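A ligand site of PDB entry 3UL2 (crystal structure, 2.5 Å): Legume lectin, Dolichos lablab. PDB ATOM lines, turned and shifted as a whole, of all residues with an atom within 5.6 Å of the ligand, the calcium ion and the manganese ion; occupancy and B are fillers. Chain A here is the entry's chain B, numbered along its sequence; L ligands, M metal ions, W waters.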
ATOM      1  N   ALA A 107      -8.290  33.580  -7.019  1.00  0.00           N
ATOM      2  CA  ALA A 107      -7.952  32.356  -6.325  1.00  0.00           C
ATOM      3  C   ALA A 107      -7.874  32.712  -4.843  1.00  0.00           C
ATOM      4  O   ALA A 107      -7.643  33.876  -4.531  1.00  0.00           O
ATOM      5  CB  ALA A 107      -6.601  31.824  -6.822  1.00  0.00           C
ATOM      6  N   ASP A 108      -8.065  31.753  -3.940  1.00  0.00           N
ATOM      7  CA  ASP A 108      -8.271  30.340  -4.261  1.00  0.00           C
ATOM      8  C   ASP A 108      -9.618  29.817  -3.804  1.00  0.00           C
ATOM      9  O   ASP A 108     -10.157  28.876  -4.384  1.00  0.00           O
ATOM     10  CB  ASP A 108      -7.155  29.499  -3.658  1.00  0.00           C
ATOM     11  CG  ASP A 108      -6.007  29.287  -4.619  1.00  0.00           C
ATOM     12  OD1 ASP A 108      -6.145  28.419  -5.515  1.00  0.00           O
ATOM     13  OD2 ASP A 108      -4.987  29.994  -4.477  1.00  0.00           O
ATOM     14  N   GLY A 125      -2.508  28.834  -0.913  1.00  0.00           N
ATOM     15  CA  GLY A 125      -2.992  28.706  -2.284  1.00  0.00           C
ATOM     16  C   GLY A 125      -4.132  27.705  -2.419  1.00  0.00           C
ATOM     17  O   GLY A 125      -5.081  27.710  -1.631  1.00  0.00           O
ATOM     18  N   GLY A 126      -4.010  26.828  -3.422  1.00  0.00           N
ATOM     19  CA  GLY A 126      -5.029  25.824  -3.738  1.00  0.00           C
ATOM     20  C   GLY A 126      -5.343  24.819  -2.643  1.00  0.00           C
ATOM     21  O   GLY A 126      -6.387  24.175  -2.684  1.00  0.00           O
ATOM     22  N   PHE A 127      -4.448  24.695  -1.659  1.00  0.00           N
ATOM     23  CA  PHE A 127      -4.660  23.811  -0.517  1.00  0.00           C
ATOM     24  C   PHE A 127      -5.534  24.449   0.581  1.00  0.00           C
ATOM     25  O   PHE A 127      -5.881  23.789   1.568  1.00  0.00           O
ATOM     26  CB  PHE A 127      -3.322  23.326   0.050  1.00  0.00           C
ATOM     27  CG  PHE A 127      -2.529  22.495  -0.913  1.00  0.00           C
ATOM     28  CD1 PHE A 127      -2.769  21.120  -1.025  1.00  0.00           C
ATOM     29  CD2 PHE A 127      -1.565  23.068  -1.725  1.00  0.00           C
ATOM     30  CE1 PHE A 127      -2.044  20.346  -1.922  1.00  0.00           C
ATOM     31  CE2 PHE A 127      -0.831  22.303  -2.628  1.00  0.00           C
ATOM     32  CZ  PHE A 127      -1.074  20.934  -2.719  1.00  0.00           C
ATOM     33  N   GLU A 146     -15.545  22.832   0.950  1.00  0.00           N
ATOM     34  CA  GLU A 146     -14.837  23.897   0.246  1.00  0.00           C
ATOM     35  C   GLU A 146     -15.729  24.598  -0.769  1.00  0.00           C
ATOM     36  O   GLU A 146     -16.657  24.012  -1.316  1.00  0.00           O
ATOM     37  CB  GLU A 146     -13.567  23.365  -0.438  1.00  0.00           C
ATOM     38  CG  GLU A 146     -13.813  22.305  -1.513  1.00  0.00           C
ATOM     39  CD  GLU A 146     -12.576  21.999  -2.333  1.00  0.00           C
ATOM     40  OE1 GLU A 146     -11.491  21.800  -1.754  1.00  0.00           O
ATOM     41  OE2 GLU A 146     -12.696  21.945  -3.576  1.00  0.00           O
ATOM     42  N   ASP A 148     -14.622  26.457  -3.943  1.00  0.00           N
ATOM     43  CA  ASP A 148     -13.352  26.520  -4.672  1.00  0.00           C
ATOM     44  C   ASP A 148     -13.465  27.374  -5.933  1.00  0.00           C
ATOM     45  O   ASP A 148     -14.084  26.959  -6.915  1.00  0.00           O
ATOM     46  CB  ASP A 148     -12.893  25.104  -4.992  1.00  0.00           C
ATOM     47  CG  ASP A 148     -11.448  25.025  -5.426  1.00  0.00           C
ATOM     48  OD1 ASP A 148     -10.868  26.026  -5.888  1.00  0.00           O
ATOM     49  OD2 ASP A 148     -10.876  23.918  -5.324  1.00  0.00           O
ATOM     50  N   THR A 149     -12.853  28.562  -5.886  1.00  0.00           N
ATOM     51  CA  THR A 149     -12.906  29.574  -6.944  1.00  0.00           C
ATOM     52  C   THR A 149     -11.889  29.326  -8.069  1.00  0.00           C
ATOM     53  O   THR A 149     -11.934  29.996  -9.097  1.00  0.00           O
ATOM     54  CB  THR A 149     -12.572  31.005  -6.391  1.00  0.00           C
ATOM     55  OG1 THR A 149     -13.510  31.397  -5.390  1.00  0.00           O
ATOM     56  CG2 THR A 149     -12.540  32.048  -7.484  1.00  0.00           C
ATOM     57  N   PHE A 150     -10.966  28.386  -7.875  1.00  0.00           N
ATOM     58  CA  PHE A 150      -9.846  28.232  -8.807  1.00  0.00           C
ATOM     59  C   PHE A 150      -9.564  26.793  -9.245  1.00  0.00           C
ATOM     60  O   PHE A 150      -9.441  25.888  -8.429  1.00  0.00           O
ATOM     61  CB  PHE A 150      -8.577  28.850  -8.222  1.00  0.00           C
ATOM     62  CG  PHE A 150      -7.415  28.855  -9.171  1.00  0.00           C
ATOM     63  CD1 PHE A 150      -6.517  27.798  -9.181  1.00  0.00           C
ATOM     64  CD2 PHE A 150      -7.232  29.901 -10.058  1.00  0.00           C
ATOM     65  CE1 PHE A 150      -5.454  27.787 -10.071  1.00  0.00           C
ATOM     66  CE2 PHE A 150      -6.165  29.902 -10.941  1.00  0.00           C
ATOM     67  CZ  PHE A 150      -5.267  28.845 -10.951  1.00  0.00           C
ATOM     68  N   TYR A 151      -9.433  26.634 -10.561  1.00  0.00           N
ATOM     69  CA  TYR A 151      -9.162  25.370 -11.217  1.00  0.00           C
ATOM     70  C   TYR A 151      -7.701  24.936 -11.006  1.00  0.00           C
ATOM     71  O   TYR A 151      -6.790  25.406 -11.691  1.00  0.00           O
ATOM     72  CB  TYR A 151      -9.488  25.531 -12.707  1.00  0.00           C
ATOM     73  CG  TYR A 151      -9.367  24.307 -13.612  1.00  0.00           C
ATOM     74  CD1 TYR A 151      -9.630  23.017 -13.130  1.00  0.00           C
ATOM     75  CD2 TYR A 151      -9.049  24.454 -14.962  1.00  0.00           C
ATOM     76  CE1 TYR A 151      -9.543  21.900 -13.972  1.00  0.00           C
ATOM     77  CE2 TYR A 151      -8.970  23.358 -15.806  1.00  0.00           C
ATOM     78  CZ  TYR A 151      -9.217  22.081 -15.311  1.00  0.00           C
ATOM     79  OH  TYR A 151      -9.126  20.995 -16.150  1.00  0.00           O
ATOM     80  N   ASN A 152      -7.496  24.044 -10.038  1.00  0.00           N
ATOM     81  CA  ASN A 152      -6.157  23.525  -9.755  1.00  0.00           C
ATOM     82  C   ASN A 152      -5.812  22.293 -10.584  1.00  0.00           C
ATOM     83  O   ASN A 152      -4.660  21.861 -10.613  1.00  0.00           O
ATOM     84  CB  ASN A 152      -5.970  23.234  -8.266  1.00  0.00           C
ATOM     85  CG  ASN A 152      -5.637  24.476  -7.465  1.00  0.00           C
ATOM     86  OD1 ASN A 152      -6.495  25.048  -6.791  1.00  0.00           O
ATOM     87  ND2 ASN A 152      -4.385  24.905  -7.535  1.00  0.00           N
ATOM     88  N   TRP A 155      -6.104  18.262  -9.349  1.00  0.00           N
ATOM     89  CA  TRP A 155      -7.130  17.553  -8.593  1.00  0.00           C
ATOM     90  C   TRP A 155      -8.561  18.070  -8.801  1.00  0.00           C
ATOM     91  O   TRP A 155      -9.516  17.364  -8.480  1.00  0.00           O
ATOM     92  CB  TRP A 155      -6.766  17.567  -7.101  1.00  0.00           C
ATOM     93  CG  TRP A 155      -6.623  18.941  -6.503  1.00  0.00           C
ATOM     94  CD1 TRP A 155      -7.624  19.731  -6.011  1.00  0.00           C
ATOM     95  CD2 TRP A 155      -5.406  19.676  -6.314  1.00  0.00           C
ATOM     96  NE1 TRP A 155      -7.107  20.915  -5.541  1.00  0.00           N
ATOM     97  CE2 TRP A 155      -5.750  20.898  -5.710  1.00  0.00           C
ATOM     98  CE3 TRP A 155      -4.060  19.415  -6.610  1.00  0.00           C
ATOM     99  CZ2 TRP A 155      -4.792  21.866  -5.377  1.00  0.00           C
ATOM    100  CZ3 TRP A 155      -3.105  20.372  -6.283  1.00  0.00           C
ATOM    101  CH2 TRP A 155      -3.478  21.587  -5.667  1.00  0.00           C
ATOM    102  N   ASP A 156      -8.705  19.274  -9.340  1.00  0.00           N
ATOM    103  CA  ASP A 156     -10.006  19.950  -9.422  1.00  0.00           C
ATOM    104  C   ASP A 156     -10.846  19.615 -10.659  1.00  0.00           C
ATOM    105  O   ASP A 156     -10.299  19.282 -11.712  1.00  0.00           O
ATOM    106  CB  ASP A 156      -9.830  21.460  -9.351  1.00  0.00           C
ATOM    107  CG  ASP A 156      -9.714  21.977  -7.928  1.00  0.00           C
ATOM    108  OD1 ASP A 156     -10.193  21.308  -6.990  1.00  0.00           O
ATOM    109  OD2 ASP A 156      -9.141  23.072  -7.749  1.00  0.00           O
ATOM    110  N   PRO A 157     -12.189  19.714 -10.534  1.00  0.00           N
ATOM    111  CA  PRO A 157     -13.079  19.714 -11.698  1.00  0.00           C
ATOM    112  C   PRO A 157     -12.888  20.995 -12.499  1.00  0.00           C
ATOM    113  O   PRO A 157     -12.251  21.925 -12.004  1.00  0.00           O
ATOM    114  CB  PRO A 157     -14.481  19.678 -11.092  1.00  0.00           C
ATOM    115  CG  PRO A 157     -14.299  19.257  -9.679  1.00  0.00           C
ATOM    116  CD  PRO A 157     -12.958  19.772  -9.269  1.00  0.00           C
ATOM    117  N   HIS A 161     -16.595  25.053  -8.001  1.00  0.00           N
ATOM    118  CA  HIS A 161     -17.292  23.939  -7.377  1.00  0.00           C
ATOM    119  C   HIS A 161     -17.384  24.031  -5.854  1.00  0.00           C
ATOM    120  O   HIS A 161     -16.598  24.720  -5.184  1.00  0.00           O
ATOM    121  CB  HIS A 161     -16.615  22.624  -7.772  1.00  0.00           C
ATOM    122  CG  HIS A 161     -15.157  22.563  -7.448  1.00  0.00           C
ATOM    123  ND1 HIS A 161     -14.192  23.163  -8.234  1.00  0.00           N
ATOM    124  CD2 HIS A 161     -14.493  21.982  -6.424  1.00  0.00           C
ATOM    125  CE1 HIS A 161     -13.000  22.959  -7.711  1.00  0.00           C
ATOM    126  NE2 HIS A 161     -13.149  22.237  -6.616  1.00  0.00           N
ATOM    127  N   ILE A 169      -7.113  17.572  -0.172  1.00  0.00           N
ATOM    128  CA  ILE A 169      -7.621  18.668  -0.995  1.00  0.00           C
ATOM    129  C   ILE A 169      -8.380  18.149  -2.219  1.00  0.00           C
ATOM    130  O   ILE A 169      -9.131  18.889  -2.870  1.00  0.00           O
ATOM    131  CB  ILE A 169      -6.495  19.673  -1.429  1.00  0.00           C
ATOM    132  CG1 ILE A 169      -7.085  20.993  -1.949  1.00  0.00           C
ATOM    133  CG2 ILE A 169      -5.561  19.046  -2.474  1.00  0.00           C
ATOM    134  CD1 ILE A 169      -7.851  21.797  -0.925  1.00  0.00           C
ATOM    135  N   SER A 171     -11.284  16.526  -3.362  1.00  0.00           N
ATOM    136  CA  SER A 171     -12.633  16.261  -2.853  1.00  0.00           C
ATOM    137  C   SER A 171     -13.113  14.854  -3.178  1.00  0.00           C
ATOM    138  O   SER A 171     -12.860  14.332  -4.272  1.00  0.00           O
ATOM    139  CB  SER A 171     -13.635  17.273  -3.413  1.00  0.00           C
ATOM    140  OG  SER A 171     -13.247  18.605  -3.159  1.00  0.00           O
ATOM    141  N   THR A 174     -17.878  16.434  -5.610  1.00  0.00           N
ATOM    142  CA  THR A 174     -18.079  17.860  -5.898  1.00  0.00           C
ATOM    143  C   THR A 174     -19.415  18.122  -6.589  1.00  0.00           C
ATOM    144  O   THR A 174     -20.106  17.175  -6.986  1.00  0.00           O
ATOM    145  CB  THR A 174     -16.958  18.473  -6.794  1.00  0.00           C
ATOM    146  OG1 THR A 174     -17.013  17.889  -8.104  1.00  0.00           O
ATOM    147  CG2 THR A 174     -15.577  18.266  -6.174  1.00  0.00           C
ATOM    148  N   THR A 235      -5.731  33.430  -0.812  1.00  0.00           N
ATOM    149  CA  THR A 235      -5.683  34.098  -2.109  1.00  0.00           C
ATOM    150  C   THR A 235      -4.606  33.421  -2.954  1.00  0.00           C
ATOM    151  O   THR A 235      -3.899  32.533  -2.461  1.00  0.00           O
ATOM    152  CB  THR A 235      -5.425  35.619  -1.981  1.00  0.00           C
ATOM    153  OG1 THR A 235      -4.189  35.852  -1.290  1.00  0.00           O
ATOM    154  CG2 THR A 235      -6.568  36.275  -1.238  1.00  0.00           C
ATOM    155  N   GLY A 236      -4.498  33.829  -4.215  1.00  0.00           N
ATOM    156  CA  GLY A 236      -3.615  33.169  -5.181  1.00  0.00           C
ATOM    157  C   GLY A 236      -2.129  33.218  -4.869  1.00  0.00           C
ATOM    158  O   GLY A 236      -1.676  34.029  -4.058  1.00  0.00           O
ATOM    159  N   LEU A 237      -1.380  32.325  -5.522  1.00  0.00           N
ATOM    160  CA  LEU A 237       0.075  32.335  -5.428  1.00  0.00           C
ATOM    161  C   LEU A 237       0.704  33.123  -6.594  1.00  0.00           C
ATOM    162  O   LEU A 237       1.838  32.865  -6.990  1.00  0.00           O
ATOM    163  CB  LEU A 237       0.624  30.911  -5.367  1.00  0.00           C
ATOM    164  CG  LEU A 237       1.987  30.694  -4.706  1.00  0.00           C
ATOM    165  CD1 LEU A 237       2.000  31.166  -3.260  1.00  0.00           C
ATOM    166  CD2 LEU A 237       2.326  29.228  -4.758  1.00  0.00           C
ATOM    167  N   SER A 238      -0.069  34.062  -7.141  1.00  0.00           N
ATOM    168  CA  SER A 238       0.439  35.020  -8.109  1.00  0.00           C
ATOM    169  C   SER A 238      -0.128  36.404  -7.852  1.00  0.00           C
ATOM    170  O   SER A 238      -1.290  36.546  -7.475  1.00  0.00           O
ATOM    171  CB  SER A 238       0.129  34.579  -9.536  1.00  0.00           C
ATOM    172  OG  SER A 238       0.733  33.333  -9.814  1.00  0.00           O
ATOM    173  N   TYR A 241      -3.813  37.228  -8.997  1.00  0.00           N
ATOM    174  CA  TYR A 241      -4.915  36.319  -8.679  1.00  0.00           C
ATOM    175  C   TYR A 241      -5.450  36.570  -7.267  1.00  0.00           C
ATOM    176  O   TYR A 241      -5.127  35.857  -6.314  1.00  0.00           O
ATOM    177  CB  TYR A 241      -4.486  34.859  -8.882  1.00  0.00           C
ATOM    178  CG  TYR A 241      -4.438  34.461 -10.355  1.00  0.00           C
ATOM    179  CD1 TYR A 241      -3.459  34.994 -11.207  1.00  0.00           C
ATOM    180  CD2 TYR A 241      -5.368  33.580 -10.890  1.00  0.00           C
ATOM    181  CE1 TYR A 241      -3.416  34.647 -12.548  1.00  0.00           C
ATOM    182  CE2 TYR A 241      -5.338  33.221 -12.235  1.00  0.00           C
ATOM    183  CZ  TYR A 241      -4.350  33.761 -13.060  1.00  0.00           C
ATOM    184  OH  TYR A 241      -4.294  33.425 -14.397  1.00  0.00           O
HETATM  185  C1  LIG L   1      -1.015  28.237  -8.665  1.00  0.00           C
HETATM  186  C2  LIG L   1      -1.632  27.758  -7.356  1.00  0.00           C
HETATM  187  C3  LIG L   1      -3.138  28.018  -7.394  1.00  0.00           C
HETATM  188  C4  LIG L   1      -3.429  29.480  -7.714  1.00  0.00           C
HETATM  189  C5  LIG L   1      -2.614  29.955  -8.929  1.00  0.00           C
HETATM  190  C6  LIG L   1      -2.797  31.443  -9.215  1.00  0.00           C
HETATM  191  O1  LIG L   1       0.361  27.961  -8.665  1.00  0.00           O
HETATM  192  O2  LIG L   1      -1.354  26.386  -7.138  1.00  0.00           O
HETATM  193  O3  LIG L   1      -3.704  27.655  -6.160  1.00  0.00           O
HETATM  194  O4  LIG L   1      -3.158  30.276  -6.579  1.00  0.00           O
HETATM  195  O5  LIG L   1      -1.230  29.636  -8.760  1.00  0.00           O
HETATM  196  O6  LIG L   1      -1.619  31.986  -9.781  1.00  0.00           O
HETATM  197 CA    CA M   1      -8.743  24.826  -6.404  1.00  0.00          CA
HETATM  198 MN    MN M   2     -11.474  21.922  -5.316  1.00  0.00          MN
HETATM  199  O   HOH W   1      -7.995  23.740  -4.705  1.00  0.00           O
HETATM  200  O   HOH W   2      -9.969  21.111  -3.871  1.00  0.00           O
HETATM  201  O   HOH W   3      -8.376  26.927  -5.028  1.00  0.00           O
HETATM  202  O   HOH W   4     -12.041  19.786  -5.203  1.00  0.00           O
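Merely in contact with the ligand: Ala 107, Gly 125, Gly 236 and Tyr 241. Within 4 Å of the ligand: Ala 107, Asp 108, Gly 125, Gly 126, Phe 150, Asn 152, Gly 236, Leu 237, Ser 238 and Tyr 241. The nearest printed residue that does not touch the ligand is Thr 235 (4.8 Å).
The side-chain amide nitrogen (ND2) of Asn 152 is in hydrogen-bond range of an oxygen (O3) of the ligand (3.1 Å). An oxygen (O3) of the ligand lies within hydrogen-bond range of the side-chain carboxylate (OD1) of Asp 108 (2.6 Å). O6 of the ligand is in hydrogen-bond range of OG of Ser 238 (2.7 Å). N of Gly 126 is in hydrogen-bond range of O3 of the ligand. The backbone NH (N) of Leu 237 sits at hydrogen-bond distance from an oxygen (O4) of the ligand, 2.9 Å away.
The manganese ion is bound by the side-chain carboxylate (OD2) of Asp 148 (2.1 Å), the side-chain carboxylate (OE2) of Glu 146 (2.1 Å), a ring nitrogen (NE2) of His 161 (2.1 Å), the side-chain carboxylate (OD1) of Asp 156 (2.2 Å), water W4 (2.2 Å) and water W2 (2.2 Å).
Within 4 Å of the manganese ion: Glu 146, Asp 148, Asp 156 and His 161.
Water W1 lies within hydrogen-bond range of the backbone carbonyl oxygen (O) of Gly 126 (2.6 Å) and the indole nitrogen (NE1) of Trp 155 (3.1 Å). Water W2 lies within hydrogen-bond range of the backbone carbonyl oxygen (O) of Ile 169 (2.6 Å), the side-chain carboxylate (OE1) of Glu 146 (2.7 Å) and the indole nitrogen (NE1) of Trp 155 (3.3 Å).
The calcium ion is bound by water W1 (2.2 Å), the side-chain carboxylate (OD2) of Asp 156 (2.2 Å), the side-chain amide oxygen (OD1) of Asn 152 (2.3 Å), the backbone carbonyl oxygen (O) of Phe 150 (2.4 Å), the side-chain carboxylate (OD1) of Asp 148 (2.5 Å), water W3 (2.5 Å) and the side-chain carboxylate (OD2) of Asp 148 (2.6 Å).
OE2 of Glu 146 sits close to OG of Ser 171 (3.4 Å). OD1 of Asp 156 lies close to NE1 of Trp 155, at 3.4 Å. OD1 of Asp 108 lies close to N of Gly 126, at 3.4 Å. The backbone carbonyl oxygen (O) of Asp 108 lies within hydrogen-bond range of the backbone NH (N) of Thr 149 (3.1 Å). The backbone NH (N) of Gly 236 is in hydrogen-bond range of the backbone carbonyl oxygen (O) of Tyr 241, at 3.0 Å. The backbone NH (N) of Gly 236 is in hydrogen-bond range of the backbone carbonyl oxygen (O) of Ala 107, 3.2 Å away.
Of the 23 residues printed, 4 come within 4 Å of the calcium ion.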
